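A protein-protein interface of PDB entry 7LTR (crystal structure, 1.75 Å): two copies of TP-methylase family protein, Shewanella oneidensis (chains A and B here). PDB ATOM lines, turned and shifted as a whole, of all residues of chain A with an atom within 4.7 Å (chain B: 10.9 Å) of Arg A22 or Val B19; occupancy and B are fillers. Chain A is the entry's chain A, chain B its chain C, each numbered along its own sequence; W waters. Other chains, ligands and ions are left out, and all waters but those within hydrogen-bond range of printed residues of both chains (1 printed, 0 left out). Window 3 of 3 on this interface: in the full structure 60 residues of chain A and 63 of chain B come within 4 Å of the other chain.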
ATOM      1  N   ALA A  14      -5.713  34.462 -29.868  1.00  0.00           N
ATOM      2  CA  ALA A  14      -4.669  33.918 -28.963  1.00  0.00           C
ATOM      3  C   ALA A  14      -5.048  32.544 -28.389  1.00  0.00           C
ATOM      4  O   ALA A  14      -4.148  31.698 -28.279  1.00  0.00           O
ATOM      5  CB  ALA A  14      -4.375  34.904 -27.856  1.00  0.00           C
ATOM      6  N   GLY A  15      -6.308  32.328 -28.004  1.00  0.00           N
ATOM      7  CA  GLY A  15      -6.695  31.158 -27.190  1.00  0.00           C
ATOM      8  C   GLY A  15      -7.221  29.991 -28.009  1.00  0.00           C
ATOM      9  O   GLY A  15      -7.422  28.913 -27.426  1.00  0.00           O
ATOM     10  N   ILE A  17      -5.884  28.704 -30.908  1.00  0.00           N
ATOM     11  CA  ILE A  17      -4.805  27.888 -31.537  1.00  0.00           C
ATOM     12  C   ILE A  17      -4.585  26.653 -30.661  1.00  0.00           C
ATOM     13  O   ILE A  17      -4.722  26.776 -29.427  1.00  0.00           O
ATOM     14  CB  ILE A  17      -3.511  28.704 -31.713  1.00  0.00           C
ATOM     15  CG1 ILE A  17      -2.481  27.940 -32.547  1.00  0.00           C
ATOM     16  CG2 ILE A  17      -2.946  29.118 -30.365  1.00  0.00           C
ATOM     17  CD1 ILE A  17      -1.311  28.777 -33.001  1.00  0.00           C
ATOM     18  N   SER A  18      -4.283  25.507 -31.272  1.00  0.00           N
ATOM     19  CA  SER A  18      -3.887  24.257 -30.572  1.00  0.00           C
ATOM     20  C   SER A  18      -2.562  24.488 -29.844  1.00  0.00           C
ATOM     21  O   SER A  18      -1.781  25.343 -30.311  1.00  0.00           O
ATOM     22  CB  SER A  18      -3.776  23.108 -31.542  1.00  0.00           C
ATOM     23  OG  SER A  18      -5.023  22.851 -32.173  1.00  0.00           O
ATOM     24  N   VAL A  19      -2.320  23.745 -28.767  1.00  0.00           N
ATOM     25  CA  VAL A  19      -1.044  23.797 -28.000  1.00  0.00           C
ATOM     26  C   VAL A  19       0.112  23.484 -28.960  1.00  0.00           C
ATOM     27  O   VAL A  19       1.094  24.249 -28.987  1.00  0.00           O
ATOM     28  CB  VAL A  19      -1.088  22.840 -26.798  1.00  0.00           C
ATOM     29  CG1 VAL A  19       0.281  22.656 -26.171  1.00  0.00           C
ATOM     30  CG2 VAL A  19      -2.102  23.310 -25.760  1.00  0.00           C
ATOM     31  N   LEU A  20      -0.009  22.419 -29.755  1.00  0.00           N
ATOM     32  CA  LEU A  20       1.090  21.980 -30.654  1.00  0.00           C
ATOM     33  C   LEU A  20       1.303  23.016 -31.765  1.00  0.00           C
ATOM     34  O   LEU A  20       2.470  23.296 -32.087  1.00  0.00           O
ATOM     35  CB  LEU A  20       0.771  20.607 -31.243  1.00  0.00           C
ATOM     36  CG  LEU A  20       1.806  20.112 -32.252  1.00  0.00           C
ATOM     37  CD1 LEU A  20       3.151  19.887 -31.581  1.00  0.00           C
ATOM     38  CD2 LEU A  20       1.325  18.851 -32.947  1.00  0.00           C
ATOM     39  N   SER A  21       0.227  23.566 -32.330  1.00  0.00           N
ATOM     40  CA  SER A  21       0.291  24.588 -33.411  1.00  0.00           C
ATOM     41  C   SER A  21       1.017  25.837 -32.904  1.00  0.00           C
ATOM     42  O   SER A  21       1.830  26.406 -33.662  1.00  0.00           O
ATOM     43  CB  SER A  21      -1.072  24.907 -33.947  1.00  0.00           C
ATOM     44  OG  SER A  21      -1.545  23.839 -34.750  1.00  0.00           O
ATOM     45  N   ARG A  22       0.754  26.253 -31.663  1.00  0.00           N
ATOM     46  CA  ARG A  22       1.446  27.414 -31.046  1.00  0.00           C
ATOM     47  C   ARG A  22       2.941  27.099 -30.925  1.00  0.00           C
ATOM     48  O   ARG A  22       3.768  28.003 -31.184  1.00  0.00           O
ATOM     49  CB  ARG A  22       0.825  27.739 -29.685  1.00  0.00           C
ATOM     50  CG  ARG A  22       1.404  28.984 -29.028  1.00  0.00           C
ATOM     51  CD  ARG A  22       0.828  29.205 -27.644  1.00  0.00           C
ATOM     52  NE  ARG A  22       1.075  30.546 -27.135  1.00  0.00           N
ATOM     53  CZ  ARG A  22       2.205  30.940 -26.557  1.00  0.00           C
ATOM     54  NH1 ARG A  22       3.214  30.096 -26.423  1.00  0.00           N
ATOM     55  NH2 ARG A  22       2.322  32.181 -26.119  1.00  0.00           N
ATOM     56  N   SER A  23       3.270  25.859 -30.557  1.00  0.00           N
ATOM     57  CA  SER A  23       4.662  25.368 -30.411  1.00  0.00           C
ATOM     58  C   SER A  23       5.384  25.453 -31.766  1.00  0.00           C
ATOM     59  O   SER A  23       6.544  25.900 -31.790  1.00  0.00           O
ATOM     60  CB  SER A  23       4.683  23.973 -29.846  1.00  0.00           C
ATOM     61  OG  SER A  23       6.014  23.559 -29.593  1.00  0.00           O
ATOM     62  N   TYR A  24       4.720  25.083 -32.865  1.00  0.00           N
ATOM     63  CA  TYR A  24       5.311  25.158 -34.228  1.00  0.00           C
ATOM     64  C   TYR A  24       5.666  26.609 -34.557  1.00  0.00           C
ATOM     65  O   TYR A  24       6.771  26.845 -35.072  1.00  0.00           O
ATOM     66  CB  TYR A  24       4.380  24.572 -35.289  1.00  0.00           C
ATOM     67  CG  TYR A  24       4.598  23.099 -35.503  1.00  0.00           C
ATOM     68  CD1 TYR A  24       5.763  22.633 -36.090  1.00  0.00           C
ATOM     69  CD2 TYR A  24       3.657  22.172 -35.098  1.00  0.00           C
ATOM     70  CE1 TYR A  24       5.984  21.281 -36.277  1.00  0.00           C
ATOM     71  CE2 TYR A  24       3.861  20.815 -35.279  1.00  0.00           C
ATOM     72  CZ  TYR A  24       5.027  20.368 -35.872  1.00  0.00           C
ATOM     73  OH  TYR A  24       5.237  19.031 -36.052  1.00  0.00           O
ATOM     74  N   ILE A  25       4.759  27.545 -34.273  1.00  0.00           N
ATOM     75  CA  ILE A  25       4.977  28.996 -34.546  1.00  0.00           C
ATOM     76  C   ILE A  25       6.180  29.457 -33.717  1.00  0.00           C
ATOM     77  O   ILE A  25       7.071  30.123 -34.277  1.00  0.00           O
ATOM     78  CB  ILE A  25       3.707  29.820 -34.255  1.00  0.00           C
ATOM     79  CG1 ILE A  25       2.576  29.466 -35.225  1.00  0.00           C
ATOM     80  CG2 ILE A  25       4.018  31.308 -34.270  1.00  0.00           C
ATOM     81  CD1 ILE A  25       1.288  30.221 -34.981  1.00  0.00           C
ATOM     82  N   GLU A  26       6.214  29.076 -32.439  1.00  0.00           N
ATOM     83  CA  GLU A  26       7.243  29.508 -31.462  1.00  0.00           C
ATOM     84  C   GLU A  26       8.636  29.102 -31.960  1.00  0.00           C
ATOM     85  O   GLU A  26       9.569  29.914 -31.832  1.00  0.00           O
ATOM     86  CB  GLU A  26       6.954  28.886 -30.096  1.00  0.00           C
ATOM     87  CG  GLU A  26       7.877  29.381 -29.001  1.00  0.00           C
ATOM     88  CD  GLU A  26       7.687  28.668 -27.673  1.00  0.00           C
ATOM     89  OE1 GLU A  26       6.601  28.086 -27.468  1.00  0.00           O
ATOM     90  OE2 GLU A  26       8.629  28.685 -26.855  1.00  0.00           O
ATOM     91  N   LEU A  47       4.973  36.118 -30.207  1.00  0.00           N
ATOM     92  CA  LEU A  47       5.276  34.661 -30.219  1.00  0.00           C
ATOM     93  C   LEU A  47       6.561  34.414 -31.010  1.00  0.00           C
ATOM     94  O   LEU A  47       7.405  33.630 -30.543  1.00  0.00           O
ATOM     95  CB  LEU A  47       4.114  33.913 -30.874  1.00  0.00           C
ATOM     96  CG  LEU A  47       3.359  32.938 -29.977  1.00  0.00           C
ATOM     97  CD1 LEU A  47       2.326  32.172 -30.789  1.00  0.00           C
ATOM     98  CD2 LEU A  47       4.320  31.981 -29.286  1.00  0.00           C
ATOM     99  N   VAL B   5     -18.467  25.129 -18.339  1.00  0.00           N
ATOM    100  CA  VAL B   5     -17.812  25.243 -19.671  1.00  0.00           C
ATOM    101  C   VAL B   5     -17.514  23.829 -20.168  1.00  0.00           C
ATOM    102  O   VAL B   5     -16.858  23.067 -19.431  1.00  0.00           O
ATOM    103  CB  VAL B   5     -16.545  26.114 -19.628  1.00  0.00           C
ATOM    104  CG1 VAL B   5     -15.926  26.237 -21.012  1.00  0.00           C
ATOM    105  CG2 VAL B   5     -16.828  27.489 -19.037  1.00  0.00           C
ATOM    106  N   VAL B   7     -15.513  21.752 -23.021  1.00  0.00           N
ATOM    107  CA  VAL B   7     -14.353  21.889 -23.945  1.00  0.00           C
ATOM    108  C   VAL B   7     -14.093  20.535 -24.606  1.00  0.00           C
ATOM    109  O   VAL B   7     -14.498  19.499 -24.039  1.00  0.00           O
ATOM    110  CB  VAL B   7     -13.104  22.416 -23.212  1.00  0.00           C
ATOM    111  CG1 VAL B   7     -13.382  23.735 -22.503  1.00  0.00           C
ATOM    112  CG2 VAL B   7     -12.546  21.388 -22.240  1.00  0.00           C
ATOM    113  N   GLY B   8     -13.445  20.567 -25.772  1.00  0.00           N
ATOM    114  CA  GLY B   8     -12.954  19.380 -26.488  1.00  0.00           C
ATOM    115  C   GLY B   8     -11.443  19.300 -26.403  1.00  0.00           C
ATOM    116  O   GLY B   8     -10.801  20.363 -26.289  1.00  0.00           O
ATOM    117  N   THR B   9     -10.888  18.088 -26.426  1.00  0.00           N
ATOM    118  CA  THR B   9      -9.423  17.848 -26.360  1.00  0.00           C
ATOM    119  C   THR B   9      -8.860  17.675 -27.773  1.00  0.00           C
ATOM    120  O   THR B   9      -7.642  17.471 -27.895  1.00  0.00           O
ATOM    121  CB  THR B   9      -9.095  16.615 -25.510  1.00  0.00           C
ATOM    122  OG1 THR B   9      -9.677  15.483 -26.157  1.00  0.00           O
ATOM    123  CG2 THR B   9      -9.599  16.724 -24.088  1.00  0.00           C
ATOM    124  N   GLY B  10      -9.708  17.744 -28.801  1.00  0.00           N
ATOM    125  CA  GLY B  10      -9.349  17.289 -30.159  1.00  0.00           C
ATOM    126  C   GLY B  10      -9.123  15.784 -30.172  1.00  0.00           C
ATOM    127  O   GLY B  10      -9.620  15.109 -29.254  1.00  0.00           O
ATOM    128  N   ALA B  14      -2.827  15.549 -25.917  1.00  0.00           N
ATOM    129  CA  ALA B  14      -2.134  16.690 -25.270  1.00  0.00           C
ATOM    130  C   ALA B  14      -2.052  17.914 -26.191  1.00  0.00           C
ATOM    131  O   ALA B  14      -2.224  19.036 -25.680  1.00  0.00           O
ATOM    132  CB  ALA B  14      -0.759  16.264 -24.822  1.00  0.00           C
ATOM    133  N   GLY B  15      -1.763  17.722 -27.482  1.00  0.00           N
ATOM    134  CA  GLY B  15      -1.318  18.813 -28.372  1.00  0.00           C
ATOM    135  C   GLY B  15      -2.452  19.503 -29.109  1.00  0.00           C
ATOM    136  O   GLY B  15      -2.238  20.643 -29.574  1.00  0.00           O
ATOM    137  N   GLN B  16      -3.618  18.864 -29.224  1.00  0.00           N
ATOM    138  CA  GLN B  16      -4.685  19.320 -30.157  1.00  0.00           C
ATOM    139  C   GLN B  16      -5.755  20.127 -29.411  1.00  0.00           C
ATOM    140  O   GLN B  16      -6.635  20.712 -30.077  1.00  0.00           O
ATOM    141  CB  GLN B  16      -5.295  18.128 -30.890  1.00  0.00           C
ATOM    142  CG  GLN B  16      -5.628  18.443 -32.338  1.00  0.00           C
ATOM    143  CD  GLN B  16      -5.717  17.203 -33.193  1.00  0.00           C
ATOM    144  OE1 GLN B  16      -6.440  16.262 -32.879  1.00  0.00           O
ATOM    145  NE2 GLN B  16      -4.980  17.200 -34.290  1.00  0.00           N
ATOM    146  N   ILE B  17      -5.686  20.179 -28.084  1.00  0.00           N
ATOM    147  CA  ILE B  17      -6.598  21.043 -27.283  1.00  0.00           C
ATOM    148  C   ILE B  17      -6.201  22.500 -27.541  1.00  0.00           C
ATOM    149  O   ILE B  17      -4.995  22.762 -27.707  1.00  0.00           O
ATOM    150  CB  ILE B  17      -6.552  20.676 -25.788  1.00  0.00           C
ATOM    151  CG1 ILE B  17      -7.649  21.408 -25.010  1.00  0.00           C
ATOM    152  CG2 ILE B  17      -5.169  20.928 -25.205  1.00  0.00           C
ATOM    153  CD1 ILE B  17      -7.861  20.895 -23.609  1.00  0.00           C
ATOM    154  N   SER B  18      -7.177  23.405 -27.604  1.00  0.00           N
ATOM    155  CA  SER B  18      -6.934  24.864 -27.734  1.00  0.00           C
ATOM    156  C   SER B  18      -6.274  25.368 -26.450  1.00  0.00           C
ATOM    157  O   SER B  18      -6.517  24.781 -25.371  1.00  0.00           O
ATOM    158  CB  SER B  18      -8.201  25.628 -28.044  1.00  0.00           C
ATOM    159  OG  SER B  18      -8.935  25.898 -26.857  1.00  0.00           O
ATOM    160  N   VAL B  19      -5.471  26.425 -26.563  1.00  0.00           N
ATOM    161  CA  VAL B  19      -4.774  27.058 -25.410  1.00  0.00           C
ATOM    162  C   VAL B  19      -5.815  27.448 -24.351  1.00  0.00           C
ATOM    163  O   VAL B  19      -5.593  27.124 -23.168  1.00  0.00           O
ATOM    164  CB  VAL B  19      -3.928  28.260 -25.865  1.00  0.00           C
ATOM    165  CG1 VAL B  19      -3.427  29.071 -24.681  1.00  0.00           C
ATOM    166  CG2 VAL B  19      -2.767  27.819 -26.747  1.00  0.00           C
ATOM    167  N   LEU B  20      -6.915  28.100 -24.746  1.00  0.00           N
ATOM    168  CA  LEU B  20      -7.968  28.541 -23.787  1.00  0.00           C
ATOM    169  C   LEU B  20      -8.638  27.321 -23.142  1.00  0.00           C
ATOM    170  O   LEU B  20      -8.870  27.355 -21.918  1.00  0.00           O
ATOM    171  CB  LEU B  20      -9.014  29.413 -24.486  1.00  0.00           C
ATOM    172  CG  LEU B  20     -10.130  29.906 -23.563  1.00  0.00           C
ATOM    173  CD1 LEU B  20      -9.565  30.780 -22.455  1.00  0.00           C
ATOM    174  CD2 LEU B  20     -11.209  30.647 -24.337  1.00  0.00           C
ATOM    175  N   SER B  21      -8.970  26.296 -23.928  1.00  0.00           N
ATOM    176  CA  SER B  21      -9.667  25.078 -23.433  1.00  0.00           C
ATOM    177  C   SER B  21      -8.810  24.373 -22.373  1.00  0.00           C
ATOM    178  O   SER B  21      -9.374  23.917 -21.360  1.00  0.00           O
ATOM    179  CB  SER B  21     -10.045  24.166 -24.563  1.00  0.00           C
ATOM    180  OG  SER B  21     -11.095  24.742 -25.324  1.00  0.00           O
ATOM    181  N   ARG B  22      -7.493  24.304 -22.578  1.00  0.00           N
ATOM    182  CA  ARG B  22      -6.559  23.705 -21.592  1.00  0.00           C
ATOM    183  C   ARG B  22      -6.564  24.552 -20.313  1.00  0.00           C
ATOM    184  O   ARG B  22      -6.529  23.957 -19.221  1.00  0.00           O
ATOM    185  CB  ARG B  22      -5.149  23.597 -22.174  1.00  0.00           C
ATOM    186  CG  ARG B  22      -4.208  22.752 -21.330  1.00  0.00           C
ATOM    187  CD  ARG B  22      -2.773  22.872 -21.802  1.00  0.00           C
ATOM    188  NE  ARG B  22      -1.911  21.897 -21.152  1.00  0.00           N
ATOM    189  CZ  ARG B  22      -1.273  22.101 -20.005  1.00  0.00           C
ATOM    190  NH1 ARG B  22      -1.400  23.254 -19.371  1.00  0.00           N
ATOM    191  NH2 ARG B  22      -0.512  21.149 -19.495  1.00  0.00           N
ATOM    192  N   SER B  23      -6.620  25.879 -20.452  1.00  0.00           N
ATOM    193  CA  SER B  23      -6.671  26.838 -19.316  1.00  0.00           C
ATOM    194  C   SER B  23      -7.949  26.589 -18.502  1.00  0.00           C
ATOM    195  O   SER B  23      -7.872  26.582 -17.262  1.00  0.00           O
ATOM    196  CB  SER B  23      -6.577  28.266 -19.793  1.00  0.00           C
ATOM    197  OG  SER B  23      -6.485  29.163 -18.695  1.00  0.00           O
ATOM    198  N   TYR B  24      -9.082  26.360 -19.171  1.00  0.00           N
ATOM    199  CA  TYR B  24     -10.378  26.083 -18.498  1.00  0.00           C
ATOM    200  C   TYR B  24     -10.255  24.815 -17.652  1.00  0.00           C
ATOM    201  O   TYR B  24     -10.737  24.801 -16.504  1.00  0.00           O
ATOM    202  CB  TYR B  24     -11.522  25.954 -19.503  1.00  0.00           C
ATOM    203  CG  TYR B  24     -12.222  27.259 -19.774  1.00  0.00           C
ATOM    204  CD1 TYR B  24     -12.906  27.914 -18.762  1.00  0.00           C
ATOM    205  CD2 TYR B  24     -12.185  27.849 -21.025  1.00  0.00           C
ATOM    206  CE1 TYR B  24     -13.540  29.123 -18.988  1.00  0.00           C
ATOM    207  CE2 TYR B  24     -12.822  29.055 -21.268  1.00  0.00           C
ATOM    208  CZ  TYR B  24     -13.501  29.695 -20.245  1.00  0.00           C
ATOM    209  OH  TYR B  24     -14.128  30.888 -20.463  1.00  0.00           O
ATOM    210  N   ILE B  25      -9.644  23.768 -18.203  1.00  0.00           N
ATOM    211  CA  ILE B  25      -9.470  22.479 -17.471  1.00  0.00           C
ATOM    212  C   ILE B  25      -8.557  22.731 -16.263  1.00  0.00           C
ATOM    213  O   ILE B  25      -8.912  22.308 -15.143  1.00  0.00           O
ATOM    214  CB  ILE B  25      -8.930  21.371 -18.395  1.00  0.00           C
ATOM    215  CG1 ILE B  25      -9.962  20.965 -19.450  1.00  0.00           C
ATOM    216  CG2 ILE B  25      -8.473  20.175 -17.576  1.00  0.00           C
ATOM    217  CD1 ILE B  25      -9.432  20.030 -20.504  1.00  0.00           C
ATOM    218  N   GLU B  26      -7.440  23.426 -16.483  1.00  0.00           N
ATOM    219  CA  GLU B  26      -6.408  23.714 -15.452  1.00  0.00           C
ATOM    220  C   GLU B  26      -7.049  24.398 -14.236  1.00  0.00           C
ATOM    221  O   GLU B  26      -6.721  24.015 -13.094  1.00  0.00           O
ATOM    222  CB  GLU B  26      -5.315  24.593 -16.059  1.00  0.00           C
ATOM    223  CG  GLU B  26      -4.139  24.823 -15.135  1.00  0.00           C
ATOM    224  CD  GLU B  26      -3.018  25.635 -15.757  1.00  0.00           C
ATOM    225  OE1 GLU B  26      -3.169  26.045 -16.924  1.00  0.00           O
ATOM    226  OE2 GLU B  26      -2.000  25.851 -15.076  1.00  0.00           O
ATOM    227  N   HIS B  27      -7.929  25.373 -14.468  1.00  0.00           N
ATOM    228  CA  HIS B  27      -8.448  26.292 -13.419  1.00  0.00           C
ATOM    229  C   HIS B  27      -9.812  25.834 -12.892  1.00  0.00           C
ATOM    230  O   HIS B  27     -10.332  26.505 -11.986  1.00  0.00           O
ATOM    231  CB  HIS B  27      -8.473  27.728 -13.951  1.00  0.00           C
ATOM    232  CG  HIS B  27      -7.104  28.306 -14.052  1.00  0.00           C
ATOM    233  ND1 HIS B  27      -6.510  28.605 -15.262  1.00  0.00           N
ATOM    234  CD2 HIS B  27      -6.193  28.594 -13.097  1.00  0.00           C
ATOM    235  CE1 HIS B  27      -5.298  29.074 -15.046  1.00  0.00           C
ATOM    236  NE2 HIS B  27      -5.080  29.078 -13.727  1.00  0.00           N
ATOM    237  N   TRP B  43      -3.379  12.078 -18.845  1.00  0.00           N
ATOM    238  CA  TRP B  43      -3.032  13.474 -19.216  1.00  0.00           C
ATOM    239  C   TRP B  43      -3.992  14.438 -18.507  1.00  0.00           C
ATOM    240  O   TRP B  43      -3.512  15.428 -17.920  1.00  0.00           O
ATOM    241  CB  TRP B  43      -3.059  13.654 -20.739  1.00  0.00           C
ATOM    242  CG  TRP B  43      -3.152  15.084 -21.172  1.00  0.00           C
ATOM    243  CD1 TRP B  43      -2.126  15.968 -21.341  1.00  0.00           C
ATOM    244  CD2 TRP B  43      -4.357  15.801 -21.487  1.00  0.00           C
ATOM    245  NE1 TRP B  43      -2.610  17.186 -21.741  1.00  0.00           N
ATOM    246  CE2 TRP B  43      -3.975  17.113 -21.842  1.00  0.00           C
ATOM    247  CE3 TRP B  43      -5.714  15.462 -21.505  1.00  0.00           C
ATOM    248  CZ2 TRP B  43      -4.908  18.081 -22.207  1.00  0.00           C
ATOM    249  CZ3 TRP B  43      -6.633  16.420 -21.868  1.00  0.00           C
ATOM    250  CH2 TRP B  43      -6.234  17.711 -22.214  1.00  0.00           C
ATOM    251  N   LEU B  47      -3.302  17.307 -15.330  1.00  0.00           N
ATOM    252  CA  LEU B  47      -3.618  18.736 -15.582  1.00  0.00           C
ATOM    253  C   LEU B  47      -4.504  19.262 -14.444  1.00  0.00           C
ATOM    254  O   LEU B  47      -4.260  20.378 -13.956  1.00  0.00           O
ATOM    255  CB  LEU B  47      -4.322  18.835 -16.937  1.00  0.00           C
ATOM    256  CG  LEU B  47      -4.687  20.241 -17.403  1.00  0.00           C
ATOM    257  CD1 LEU B  47      -3.578  21.230 -17.082  1.00  0.00           C
ATOM    258  CD2 LEU B  47      -4.989  20.240 -18.895  1.00  0.00           C
ATOM    259  N   VAL B  89     -16.098  22.162 -15.404  1.00  0.00           N
ATOM    260  CA  VAL B  89     -15.656  21.985 -16.811  1.00  0.00           C
ATOM    261  C   VAL B  89     -15.909  20.530 -17.198  1.00  0.00           C
ATOM    262  O   VAL B  89     -15.638  19.633 -16.382  1.00  0.00           O
ATOM    263  CB  VAL B  89     -14.186  22.398 -17.004  1.00  0.00           C
ATOM    264  CG1 VAL B  89     -13.670  22.001 -18.377  1.00  0.00           C
ATOM    265  CG2 VAL B  89     -13.999  23.886 -16.762  1.00  0.00           C
ATOM    266  N   GLU B 120     -16.975  25.545 -25.845  1.00  0.00           N
ATOM    267  CA  GLU B 120     -15.768  25.950 -26.609  1.00  0.00           C
ATOM    268  C   GLU B 120     -15.576  24.964 -27.754  1.00  0.00           C
ATOM    269  O   GLU B 120     -15.489  23.759 -27.530  1.00  0.00           O
ATOM    270  CB  GLU B 120     -14.537  25.963 -25.705  1.00  0.00           C
ATOM    271  CG  GLU B 120     -14.565  27.071 -24.676  1.00  0.00           C
ATOM    272  CD  GLU B 120     -14.626  28.461 -25.286  1.00  0.00           C
ATOM    273  OE1 GLU B 120     -14.087  28.636 -26.395  1.00  0.00           O
ATOM    274  OE2 GLU B 120     -15.225  29.353 -24.662  1.00  0.00           O
ATOM    275  N   PRO B 121     -15.500  25.437 -29.015  1.00  0.00           N
ATOM    276  CA  PRO B 121     -15.279  24.534 -30.137  1.00  0.00           C
ATOM    277  C   PRO B 121     -13.913  23.856 -29.986  1.00  0.00           C
ATOM    278  O   PRO B 121     -13.029  24.426 -29.366  1.00  0.00           O
ATOM    279  CB  PRO B 121     -15.346  25.435 -31.377  1.00  0.00           C
ATOM    280  CG  PRO B 121     -15.069  26.828 -30.851  1.00  0.00           C
ATOM    281  CD  PRO B 121     -15.585  26.846 -29.424  1.00  0.00           C
ATOM    282  N   GLY B 122     -13.793  22.644 -30.527  1.00  0.00           N
ATOM    283  CA  GLY B 122     -12.539  21.875 -30.547  1.00  0.00           C
ATOM    284  C   GLY B 122     -12.311  21.273 -31.917  1.00  0.00           C
ATOM    285  O   GLY B 122     -13.197  21.409 -32.783  1.00  0.00           O
ATOM    286  N   ILE B 123     -11.164  20.628 -32.105  1.00  0.00           N
ATOM    287  CA  ILE B 123     -10.795  19.962 -33.385  1.00  0.00           C
ATOM    288  C   ILE B 123     -11.507  18.606 -33.449  1.00  0.00           C
ATOM    289  O   ILE B 123     -11.294  17.769 -32.553  1.00  0.00           O
ATOM    290  CB  ILE B 123      -9.265  19.856 -33.504  1.00  0.00           C
ATOM    291  CG1 ILE B 123      -8.658  21.241 -33.751  1.00  0.00           C
ATOM    292  CG2 ILE B 123      -8.872  18.851 -34.576  1.00  0.00           C
ATOM    293  CD1 ILE B 123      -7.180  21.329 -33.488  1.00  0.00           C
HETATM  294  O   HOH W   1     -10.599  27.933 -27.236  1.00  0.00           O
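Printed residues of chain A within 4 Å of Val B19: Gly A15 (3.3 Å), Ile A17 (3.0 Å) and Arg A22 (3.96 Å).
Gly A15 touches just these residues of chain B: Ser B18, Val B19 and Leu B20.
Ser A23 touches none of the printed residues of chain B.
No residue of chain B comes within 4 Å of Ile A25.
No residue of chain B comes within 4 Å of Glu A26.
No residue of chain B comes within 4 Å of Leu A47.
Printed residues of chain B within 4 Å of Leu A20: Gly B15.
Of the printed residues of chain A, Ser B18 touches Gly A15 and Ile A17.
The nearest printed residue of chain B that does not touch Arg A22 is Gly B15 (6.7 Å).
The nearest printed residue of chain A that does not touch Val B19 is Ala A14 (4.2 Å).
The nearest printed residue of chain B that does not touch Val A19 is Arg B22 (4.04 Å).
CA of Ser B18 touches O of Ile A17, 3.4 Å away.
CB of Ser A18 touches O of Gly B15, 3.5 Å away.
CA of Ser A18 touches O of Ile B17 (3.4 Å).
Ser A18 touches Ile B123.
Val B19 touches Arg A22.
Of the 13 printed residues of chain A, 6 touch a printed residue of chain B.
Hydrophobic or aromatic side chains of chain A within 4 Å of the printed part of chain B: Ile A17, Val A19 and Leu A20.
Printed residues of chain B that touch a printed residue of chain A: Gly B15, Gln B16, Ile B17, Ser B18, Val B19, Leu B20 and Ile B123.
Hydrophobic or aromatic side chains of chain B that line the printed part of chain A: Ile B17, Val B19, Leu B20 and Ile B123.
Along chain B the printed residues that touch a printed residue of chain A span positions 15 to 123.
Among the printed residues, 13 pairs touch across the chains.
Water W1 bridges the side-chain hydroxyl (OG) of Ser B18 (2.7 Å) and the backbone carbonyl oxygen (O) of Gly A15 (3.3 Å).
Gly A15 touches Ser B18, and with the chains exchanged Ser A18 touches Gly B15.
Ile A17 touches Ser B18, and with the chains exchanged Ser A18 touches Ile B17.
Ile A17 touches Val B19, and with the chains exchanged Val A19 touches Ile B17.
Arg A22 touches Val B19, but with the chains exchanged Val A19 does not touch Arg B22 (4.04 Å).
The backbone carbonyl oxygen (O) of Gly A15 lies within hydrogen-bond range of the backbone NH (N) of Val B19, 3.3 Å away.
The side-chain hydroxyl (OG) of Ser A18 is in hydrogen-bond range of the backbone carbonyl oxygen (O) of Gln B16 (3.4 Å).
The side-chain hydroxyl (OG) of Ser B18 lies within hydrogen-bond range of the backbone carbonyl oxygen (O) of Gly A15 (3.4 Å).
N of Val B19 is in hydrogen-bond range of O of Ile A17 (3.0 Å).
N of Val A19 lies within hydrogen-bond range of O of Gly B15 (3.2 Å).
O of Gly A15 sits at hydrogen-bond distance from N of Leu B20, 2.8 Å away.
The backbone carbonyl oxygen of Gly B15 sits at hydrogen-bond distance from the backbone NH of Leu A20, 2.9 Å away.
N of Val A19 is in hydrogen-bond range of O of Ile B17 (3.0 Å).
The side-chain hydroxyl of Ser B18 is in hydrogen-bond range of the side-chain hydroxyl of Ser B21 (2.9 Å).
The backbone carbonyl oxygen of Thr B9 is in hydrogen-bond range of the backbone NH of Ile B17 (3.3 Å).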
